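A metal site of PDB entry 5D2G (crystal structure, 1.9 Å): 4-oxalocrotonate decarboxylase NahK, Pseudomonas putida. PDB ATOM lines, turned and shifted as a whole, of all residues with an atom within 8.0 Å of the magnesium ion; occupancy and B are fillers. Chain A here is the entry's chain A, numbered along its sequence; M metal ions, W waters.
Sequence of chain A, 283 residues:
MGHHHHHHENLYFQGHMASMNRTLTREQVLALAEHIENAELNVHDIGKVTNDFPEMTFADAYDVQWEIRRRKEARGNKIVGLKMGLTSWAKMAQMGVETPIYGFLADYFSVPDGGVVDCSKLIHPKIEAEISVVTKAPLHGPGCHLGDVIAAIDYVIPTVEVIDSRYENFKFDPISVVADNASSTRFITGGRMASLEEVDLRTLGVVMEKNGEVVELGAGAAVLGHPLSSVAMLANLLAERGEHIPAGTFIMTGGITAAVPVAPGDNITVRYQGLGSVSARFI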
ATOM      1  N   LYS A  83      10.223  28.149  -0.525  1.00  0.00           N
ATOM      2  CA  LYS A  83       9.466  27.264  -1.397  1.00  0.00           C
ATOM      3  C   LYS A  83       8.140  27.904  -1.769  1.00  0.00           C
ATOM      4  O   LYS A  83       7.633  28.771  -1.073  1.00  0.00           O
ATOM      5  CB  LYS A  83       9.258  25.875  -0.748  1.00  0.00           C
ATOM      6  CG  LYS A  83       8.663  25.864   0.679  1.00  0.00           C
ATOM      7  CD  LYS A  83       7.159  26.187   0.730  1.00  0.00           C
ATOM      8  CE  LYS A  83       6.318  25.141   0.013  1.00  0.00           C
ATOM      9  NZ  LYS A  83       6.131  23.847   0.787  1.00  0.00           N
ATOM     10  N   MET A  84       7.573  27.464  -2.884  1.00  0.00           N
ATOM     11  CA  MET A  84       6.299  27.997  -3.338  1.00  0.00           C
ATOM     12  C   MET A  84       5.193  26.978  -3.195  1.00  0.00           C
ATOM     13  O   MET A  84       5.418  25.770  -3.311  1.00  0.00           O
ATOM     14  CB  MET A  84       6.413  28.433  -4.788  1.00  0.00           C
ATOM     15  CG  MET A  84       7.531  29.410  -5.021  1.00  0.00           C
ATOM     16  SD  MET A  84       7.247  30.929  -4.097  1.00  0.00           S
ATOM     17  CE  MET A  84       5.680  31.449  -4.795  1.00  0.00           C
ATOM     18  N   GLY A  85       3.974  27.481  -2.990  1.00  0.00           N
ATOM     19  CA  GLY A  85       2.798  26.628  -2.910  1.00  0.00           C
ATOM     20  C   GLY A  85       1.749  27.234  -3.818  1.00  0.00           C
ATOM     21  O   GLY A  85       1.903  28.391  -4.208  1.00  0.00           O
ATOM     22  N   LEU A  86       0.694  26.477  -4.125  1.00  0.00           N
ATOM     23  CA  LEU A  86      -0.393  26.978  -4.987  1.00  0.00           C
ATOM     24  C   LEU A  86       0.124  27.612  -6.286  1.00  0.00           C
ATOM     25  O   LEU A  86      -0.222  28.747  -6.620  1.00  0.00           O
ATOM     26  CB  LEU A  86      -1.258  27.977  -4.215  1.00  0.00           C
ATOM     27  CG  LEU A  86      -1.886  27.441  -2.930  1.00  0.00           C
ATOM     28  CD1 LEU A  86      -2.896  28.435  -2.409  1.00  0.00           C
ATOM     29  CD2 LEU A  86      -2.539  26.089  -3.182  1.00  0.00           C
ATOM     30  N   THR A  87       0.961  26.882  -7.011  1.00  0.00           N
ATOM     31  CA  THR A  87       1.578  27.428  -8.219  1.00  0.00           C
ATOM     32  C   THR A  87       0.856  26.914  -9.433  1.00  0.00           C
ATOM     33  O   THR A  87       1.420  26.825 -10.515  1.00  0.00           O
ATOM     34  CB  THR A  87       3.059  27.014  -8.322  1.00  0.00           C
ATOM     35  OG1 THR A  87       3.148  25.588  -8.244  1.00  0.00           O
ATOM     36  CG2 THR A  87       3.824  27.604  -7.160  1.00  0.00           C
ATOM     37  N   LEU A 105      12.601  27.317   3.968  1.00  0.00           N
ATOM     38  CA  LEU A 105      13.220  26.029   4.225  1.00  0.00           C
ATOM     39  C   LEU A 105      14.264  26.214   5.306  1.00  0.00           C
ATOM     40  O   LEU A 105      15.085  27.134   5.248  1.00  0.00           O
ATOM     41  CB  LEU A 105      13.859  25.471   2.952  1.00  0.00           C
ATOM     42  CG  LEU A 105      12.943  25.343   1.725  1.00  0.00           C
ATOM     43  CD1 LEU A 105      13.716  24.987   0.448  1.00  0.00           C
ATOM     44  CD2 LEU A 105      11.872  24.326   1.980  1.00  0.00           C
ATOM     45  N   ILE A 127       5.009  13.673  -1.150  1.00  0.00           N
ATOM     46  CA  ILE A 127       6.120  14.209  -1.924  1.00  0.00           C
ATOM     47  C   ILE A 127       5.569  14.833  -3.203  1.00  0.00           C
ATOM     48  O   ILE A 127       4.490  14.461  -3.663  1.00  0.00           O
ATOM     49  CB  ILE A 127       7.164  13.130  -2.254  1.00  0.00           C
ATOM     50  CG1 ILE A 127       6.524  11.951  -2.987  1.00  0.00           C
ATOM     51  CG2 ILE A 127       7.826  12.615  -0.969  1.00  0.00           C
ATOM     52  CD1 ILE A 127       7.532  11.134  -3.774  1.00  0.00           C
ATOM     53  N   GLU A 128       6.312  15.787  -3.749  1.00  0.00           N
ATOM     54  CA  GLU A 128       5.948  16.383  -5.011  1.00  0.00           C
ATOM     55  C   GLU A 128       7.252  16.698  -5.730  1.00  0.00           C
ATOM     56  O   GLU A 128       8.233  17.104  -5.088  1.00  0.00           O
ATOM     57  CB  GLU A 128       5.097  17.644  -4.775  1.00  0.00           C
ATOM     58  CG  GLU A 128       5.729  18.658  -3.847  1.00  0.00           C
ATOM     59  CD  GLU A 128       4.817  19.855  -3.528  1.00  0.00           C
ATOM     60  OE1 GLU A 128       3.688  19.957  -4.058  1.00  0.00           O
ATOM     61  OE2 GLU A 128       5.256  20.693  -2.715  1.00  0.00           O
ATOM     62  N   ALA A 129       7.295  16.454  -7.038  1.00  0.00           N
ATOM     63  CA  ALA A 129       8.493  16.725  -7.837  1.00  0.00           C
ATOM     64  C   ALA A 129       8.537  18.199  -8.207  1.00  0.00           C
ATOM     65  O   ALA A 129       7.535  18.771  -8.644  1.00  0.00           O
ATOM     66  CB  ALA A 129       8.493  15.899  -9.067  1.00  0.00           C
ATOM     67  N   GLU A 130       9.702  18.821  -8.043  1.00  0.00           N
ATOM     68  CA  GLU A 130       9.856  20.224  -8.347  1.00  0.00           C
ATOM     69  C   GLU A 130      11.181  20.520  -9.023  1.00  0.00           C
ATOM     70  O   GLU A 130      12.088  19.667  -9.078  1.00  0.00           O
ATOM     71  CB  GLU A 130       9.747  21.084  -7.073  1.00  0.00           C
ATOM     72  CG  GLU A 130       8.596  20.682  -6.137  1.00  0.00           C
ATOM     73  CD  GLU A 130       8.230  21.743  -5.129  1.00  0.00           C
ATOM     74  OE1 GLU A 130       7.503  21.391  -4.176  1.00  0.00           O
ATOM     75  OE2 GLU A 130       8.637  22.918  -5.289  1.00  0.00           O
ATOM     76  N   THR A 159      14.469  18.860  -7.461  1.00  0.00           N
ATOM     77  CA  THR A 159      14.223  18.767  -6.023  1.00  0.00           C
ATOM     78  C   THR A 159      12.856  18.155  -5.787  1.00  0.00           C
ATOM     79  O   THR A 159      11.862  18.578  -6.386  1.00  0.00           O
ATOM     80  CB  THR A 159      14.208  20.163  -5.367  1.00  0.00           C
ATOM     81  OG1 THR A 159      15.363  20.895  -5.772  1.00  0.00           O
ATOM     82  CG2 THR A 159      14.169  20.036  -3.825  1.00  0.00           C
ATOM     83  N   VAL A 160      12.790  17.176  -4.901  1.00  0.00           N
ATOM     84  CA  VAL A 160      11.513  16.657  -4.458  1.00  0.00           C
ATOM     85  C   VAL A 160      11.228  17.265  -3.101  1.00  0.00           C
ATOM     86  O   VAL A 160      12.096  17.220  -2.225  1.00  0.00           O
ATOM     87  CB  VAL A 160      11.568  15.119  -4.346  1.00  0.00           C
ATOM     88  CG1 VAL A 160      10.333  14.595  -3.623  1.00  0.00           C
ATOM     89  CG2 VAL A 160      11.728  14.496  -5.719  1.00  0.00           C
ATOM     90  N   GLU A 161      10.041  17.841  -2.916  1.00  0.00           N
ATOM     91  CA  GLU A 161       9.689  18.326  -1.586  1.00  0.00           C
ATOM     92  C   GLU A 161       8.917  17.244  -0.857  1.00  0.00           C
ATOM     93  O   GLU A 161       8.107  16.536  -1.452  1.00  0.00           O
ATOM     94  CB  GLU A 161       8.822  19.589  -1.622  1.00  0.00           C
ATOM     95  CG  GLU A 161       8.816  20.277  -0.255  1.00  0.00           C
ATOM     96  CD  GLU A 161       8.052  21.589  -0.224  1.00  0.00           C
ATOM     97  OE1 GLU A 161       7.320  21.907  -1.191  1.00  0.00           O
ATOM     98  OE2 GLU A 161       8.188  22.293   0.795  1.00  0.00           O
ATOM     99  N   VAL A 162       9.185  17.110   0.440  1.00  0.00           N
ATOM    100  CA  VAL A 162       8.289  16.330   1.263  1.00  0.00           C
ATOM    101  C   VAL A 162       7.484  17.382   1.993  1.00  0.00           C
ATOM    102  O   VAL A 162       8.051  18.199   2.735  1.00  0.00           O
ATOM    103  CB  VAL A 162       9.030  15.489   2.294  1.00  0.00           C
ATOM    104  CG1 VAL A 162       8.022  14.666   3.079  1.00  0.00           C
ATOM    105  CG2 VAL A 162      10.058  14.589   1.608  1.00  0.00           C
ATOM    106  N   ILE A 163       6.177  17.395   1.761  1.00  0.00           N
ATOM    107  CA  ILE A 163       5.336  18.354   2.471  1.00  0.00           C
ATOM    108  C   ILE A 163       4.545  17.590   3.519  1.00  0.00           C
ATOM    109  O   ILE A 163       4.298  16.401   3.354  1.00  0.00           O
ATOM    110  CB  ILE A 163       4.377  19.118   1.539  1.00  0.00           C
ATOM    111  CG1 ILE A 163       3.490  18.154   0.750  1.00  0.00           C
ATOM    112  CG2 ILE A 163       5.150  20.027   0.576  1.00  0.00           C
ATOM    113  CD1 ILE A 163       2.485  18.876  -0.177  1.00  0.00           C
ATOM    114  N   ALA A 182       3.579  26.806   4.725  1.00  0.00           N
ATOM    115  CA  ALA A 182       3.289  26.177   3.445  1.00  0.00           C
ATOM    116  C   ALA A 182       3.590  24.682   3.478  1.00  0.00           C
ATOM    117  O   ALA A 182       4.050  24.110   2.490  1.00  0.00           O
ATOM    118  CB  ALA A 182       4.050  26.866   2.307  1.00  0.00           C
ATOM    119  N   SER A 183       3.345  24.090   4.646  1.00  0.00           N
ATOM    120  CA  SER A 183       3.448  22.643   4.869  1.00  0.00           C
ATOM    121  C   SER A 183       4.864  22.105   4.628  1.00  0.00           C
ATOM    122  O   SER A 183       5.045  20.931   4.308  1.00  0.00           O
ATOM    123  CB  SER A 183       2.427  21.909   4.009  1.00  0.00           C
ATOM    124  OG  SER A 183       1.118  22.429   4.239  1.00  0.00           O
ATOM    125  N   SER A 184       5.865  22.963   4.762  1.00  0.00           N
ATOM    126  CA  SER A 184       7.198  22.522   4.430  1.00  0.00           C
ATOM    127  C   SER A 184       7.708  21.586   5.499  1.00  0.00           C
ATOM    128  O   SER A 184       7.393  21.766   6.678  1.00  0.00           O
ATOM    129  CB  SER A 184       8.144  23.711   4.290  1.00  0.00           C
ATOM    130  OG  SER A 184       7.560  24.681   3.462  1.00  0.00           O
ATOM    131  N   ARG A 186      10.557  18.633   4.475  1.00  0.00           N
ATOM    132  CA  ARG A 186      11.825  18.142   3.968  1.00  0.00           C
ATOM    133  C   ARG A 186      11.926  18.518   2.510  1.00  0.00           C
ATOM    134  O   ARG A 186      10.913  18.751   1.853  1.00  0.00           O
ATOM    135  CB  ARG A 186      11.967  16.619   4.095  1.00  0.00           C
ATOM    136  CG  ARG A 186      11.881  16.060   5.508  1.00  0.00           C
ATOM    137  CD  ARG A 186      13.129  16.349   6.333  1.00  0.00           C
ATOM    138  NE  ARG A 186      13.017  15.677   7.630  1.00  0.00           N
ATOM    139  CZ  ARG A 186      12.438  16.230   8.709  1.00  0.00           C
ATOM    140  NH1 ARG A 186      11.937  17.459   8.632  1.00  0.00           N
ATOM    141  NH2 ARG A 186      12.354  15.541   9.836  1.00  0.00           N
ATOM    142  N   PHE A 187      13.159  18.582   2.005  1.00  0.00           N
ATOM    143  CA  PHE A 187      13.365  18.682   0.578  1.00  0.00           C
ATOM    144  C   PHE A 187      14.594  17.878   0.212  1.00  0.00           C
ATOM    145  O   PHE A 187      15.566  17.828   0.966  1.00  0.00           O
ATOM    146  CB  PHE A 187      13.440  20.144   0.095  1.00  0.00           C
ATOM    147  CG  PHE A 187      14.657  20.884   0.577  1.00  0.00           C
ATOM    148  CD1 PHE A 187      14.660  21.511   1.813  1.00  0.00           C
ATOM    149  CD2 PHE A 187      15.799  20.962  -0.219  1.00  0.00           C
ATOM    150  CE1 PHE A 187      15.778  22.206   2.261  1.00  0.00           C
ATOM    151  CE2 PHE A 187      16.931  21.653   0.210  1.00  0.00           C
ATOM    152  CZ  PHE A 187      16.915  22.281   1.457  1.00  0.00           C
ATOM    153  N   MET A 252      12.423  26.623  -4.248  1.00  0.00           N
ATOM    154  CA  MET A 252      11.696  25.512  -4.841  1.00  0.00           C
ATOM    155  C   MET A 252      10.468  26.076  -5.517  1.00  0.00           C
ATOM    156  O   MET A 252       9.579  26.632  -4.859  1.00  0.00           O
ATOM    157  CB  MET A 252      11.316  24.501  -3.766  1.00  0.00           C
ATOM    158  CG  MET A 252      12.518  24.043  -2.976  1.00  0.00           C
ATOM    159  SD  MET A 252      12.107  22.690  -1.874  1.00  0.00           S
ATOM    160  CE  MET A 252      11.197  21.671  -3.022  1.00  0.00           C
ATOM    161  N   THR A 253      10.408  25.941  -6.837  1.00  0.00           N
ATOM    162  CA  THR A 253       9.445  26.710  -7.609  1.00  0.00           C
ATOM    163  C   THR A 253       8.016  26.190  -7.610  1.00  0.00           C
ATOM    164  O   THR A 253       7.114  26.894  -8.069  1.00  0.00           O
ATOM    165  CB  THR A 253       9.925  26.901  -9.052  1.00  0.00           C
ATOM    166  OG1 THR A 253      10.048  25.622  -9.692  1.00  0.00           O
ATOM    167  CG2 THR A 253      11.263  27.636  -9.057  1.00  0.00           C
ATOM    168  N   GLY A 254       7.785  24.989  -7.085  1.00  0.00           N
ATOM    169  CA  GLY A 254       6.417  24.501  -7.012  1.00  0.00           C
ATOM    170  C   GLY A 254       6.188  23.118  -7.572  1.00  0.00           C
ATOM    171  O   GLY A 254       7.078  22.546  -8.237  1.00  0.00           O
ATOM    172  N   GLY A 255       4.995  22.581  -7.309  1.00  0.00           N
ATOM    173  CA  GLY A 255       4.677  21.210  -7.636  1.00  0.00           C
ATOM    174  C   GLY A 255       4.456  20.971  -9.116  1.00  0.00           C
ATOM    175  O   GLY A 255       3.468  21.453  -9.690  1.00  0.00           O
ATOM    176  N   ILE A 256       5.370  20.236  -9.739  1.00  0.00           N
ATOM    177  CA  ILE A 256       5.213  19.830 -11.139  1.00  0.00           C
ATOM    178  C   ILE A 256       4.227  18.668 -11.216  1.00  0.00           C
ATOM    179  O   ILE A 256       3.460  18.564 -12.177  1.00  0.00           O
ATOM    180  CB  ILE A 256       6.561  19.433 -11.752  1.00  0.00           C
ATOM    181  CG1 ILE A 256       7.448  20.674 -11.898  1.00  0.00           C
ATOM    182  CG2 ILE A 256       6.379  18.758 -13.119  1.00  0.00           C
ATOM    183  CD1 ILE A 256       8.884  20.340 -12.208  1.00  0.00           C
ATOM    184  N   THR A 257       4.275  17.802 -10.206  1.00  0.00           N
ATOM    185  CA  THR A 257       3.341  16.690 -10.112  1.00  0.00           C
ATOM    186  C   THR A 257       2.407  16.954  -8.950  1.00  0.00           C
ATOM    187  O   THR A 257       2.689  17.790  -8.102  1.00  0.00           O
ATOM    188  CB  THR A 257       4.072  15.370  -9.804  1.00  0.00           C
ATOM    189  OG1 THR A 257       4.728  15.491  -8.525  1.00  0.00           O
ATOM    190  CG2 THR A 257       5.116  15.067 -10.885  1.00  0.00           C
ATOM    191  N   ALA A 259       0.840  15.882  -5.337  1.00  0.00           N
ATOM    192  CA  ALA A 259       1.553  15.395  -4.168  1.00  0.00           C
ATOM    193  C   ALA A 259       1.135  13.962  -3.901  1.00  0.00           C
ATOM    194  O   ALA A 259      -0.038  13.627  -3.998  1.00  0.00           O
ATOM    195  CB  ALA A 259       1.265  16.296  -2.969  1.00  0.00           C
HETATM  196 MG    MG M   1       6.421  22.267  -2.864  1.00  0.00          MG
HETATM  197  O   HOH W   1       4.927  22.811  -4.285  1.00  0.00           O
HETATM  198  O   HOH W   2       7.406  24.005  -3.165  1.00  0.00           O
HETATM  199  O   HOH W   3       5.019  23.275  -2.023  1.00  0.00           O
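N of Gly 254 is in hydrogen-bond range of OE2 of Glu 130, 2.9 Å away. N of Glu 130 sits at hydrogen-bond distance from O of Thr 159 (2.7 Å). The side-chain carboxylate (OE2) of Glu 161 lies within salt-bridge range of the side-chain amino group (NZ) of Lys 83 (2.6 Å). The backbone NH (N) of Met 84 lies within hydrogen-bond range of the backbone carbonyl oxygen (O) of Met 252, at 2.9 Å. The backbone carbonyl oxygen of Ala 182 lies within hydrogen-bond range of the side-chain amino group of Lys 83 (2.7 Å). NZ of Lys 83 sits at hydrogen-bond distance from OG of Ser 184 (3.1 Å).
Residues that only touch the magnesium ion: Met 84 (3.7 Å) and Lys 83 (3.99 Å). Of the 27 residues printed, 5 come within 4 Å of the magnesium ion.
The magnesium ion is bound by the side-chain carboxylate of Glu 130 (1.9 Å), water W3 (1.9 Å), the side-chain carboxylate of Glu 161 (1.9 Å), the side-chain carboxylate of Glu 128 (2.0 Å), water W2 (2.0 Å) and water W1 (2.1 Å). The magnesium ion has six donor atoms within binding distance.
Water W2 lies within hydrogen-bond range of the backbone carbonyl oxygen (O) of Met 84 (2.7 Å) and the side-chain carboxylate (OE2) of Glu 130 (2.7 Å). Water W1 lies within hydrogen-bond range of N of Gly 255 (3.0 Å), OE1 of Glu 128 (3.1 Å) and O of Met 84 (3.2 Å). Water W3 lies within hydrogen-bond range of O of Met 84 (2.8 Å) and NZ of Lys 83 (3.1 Å).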
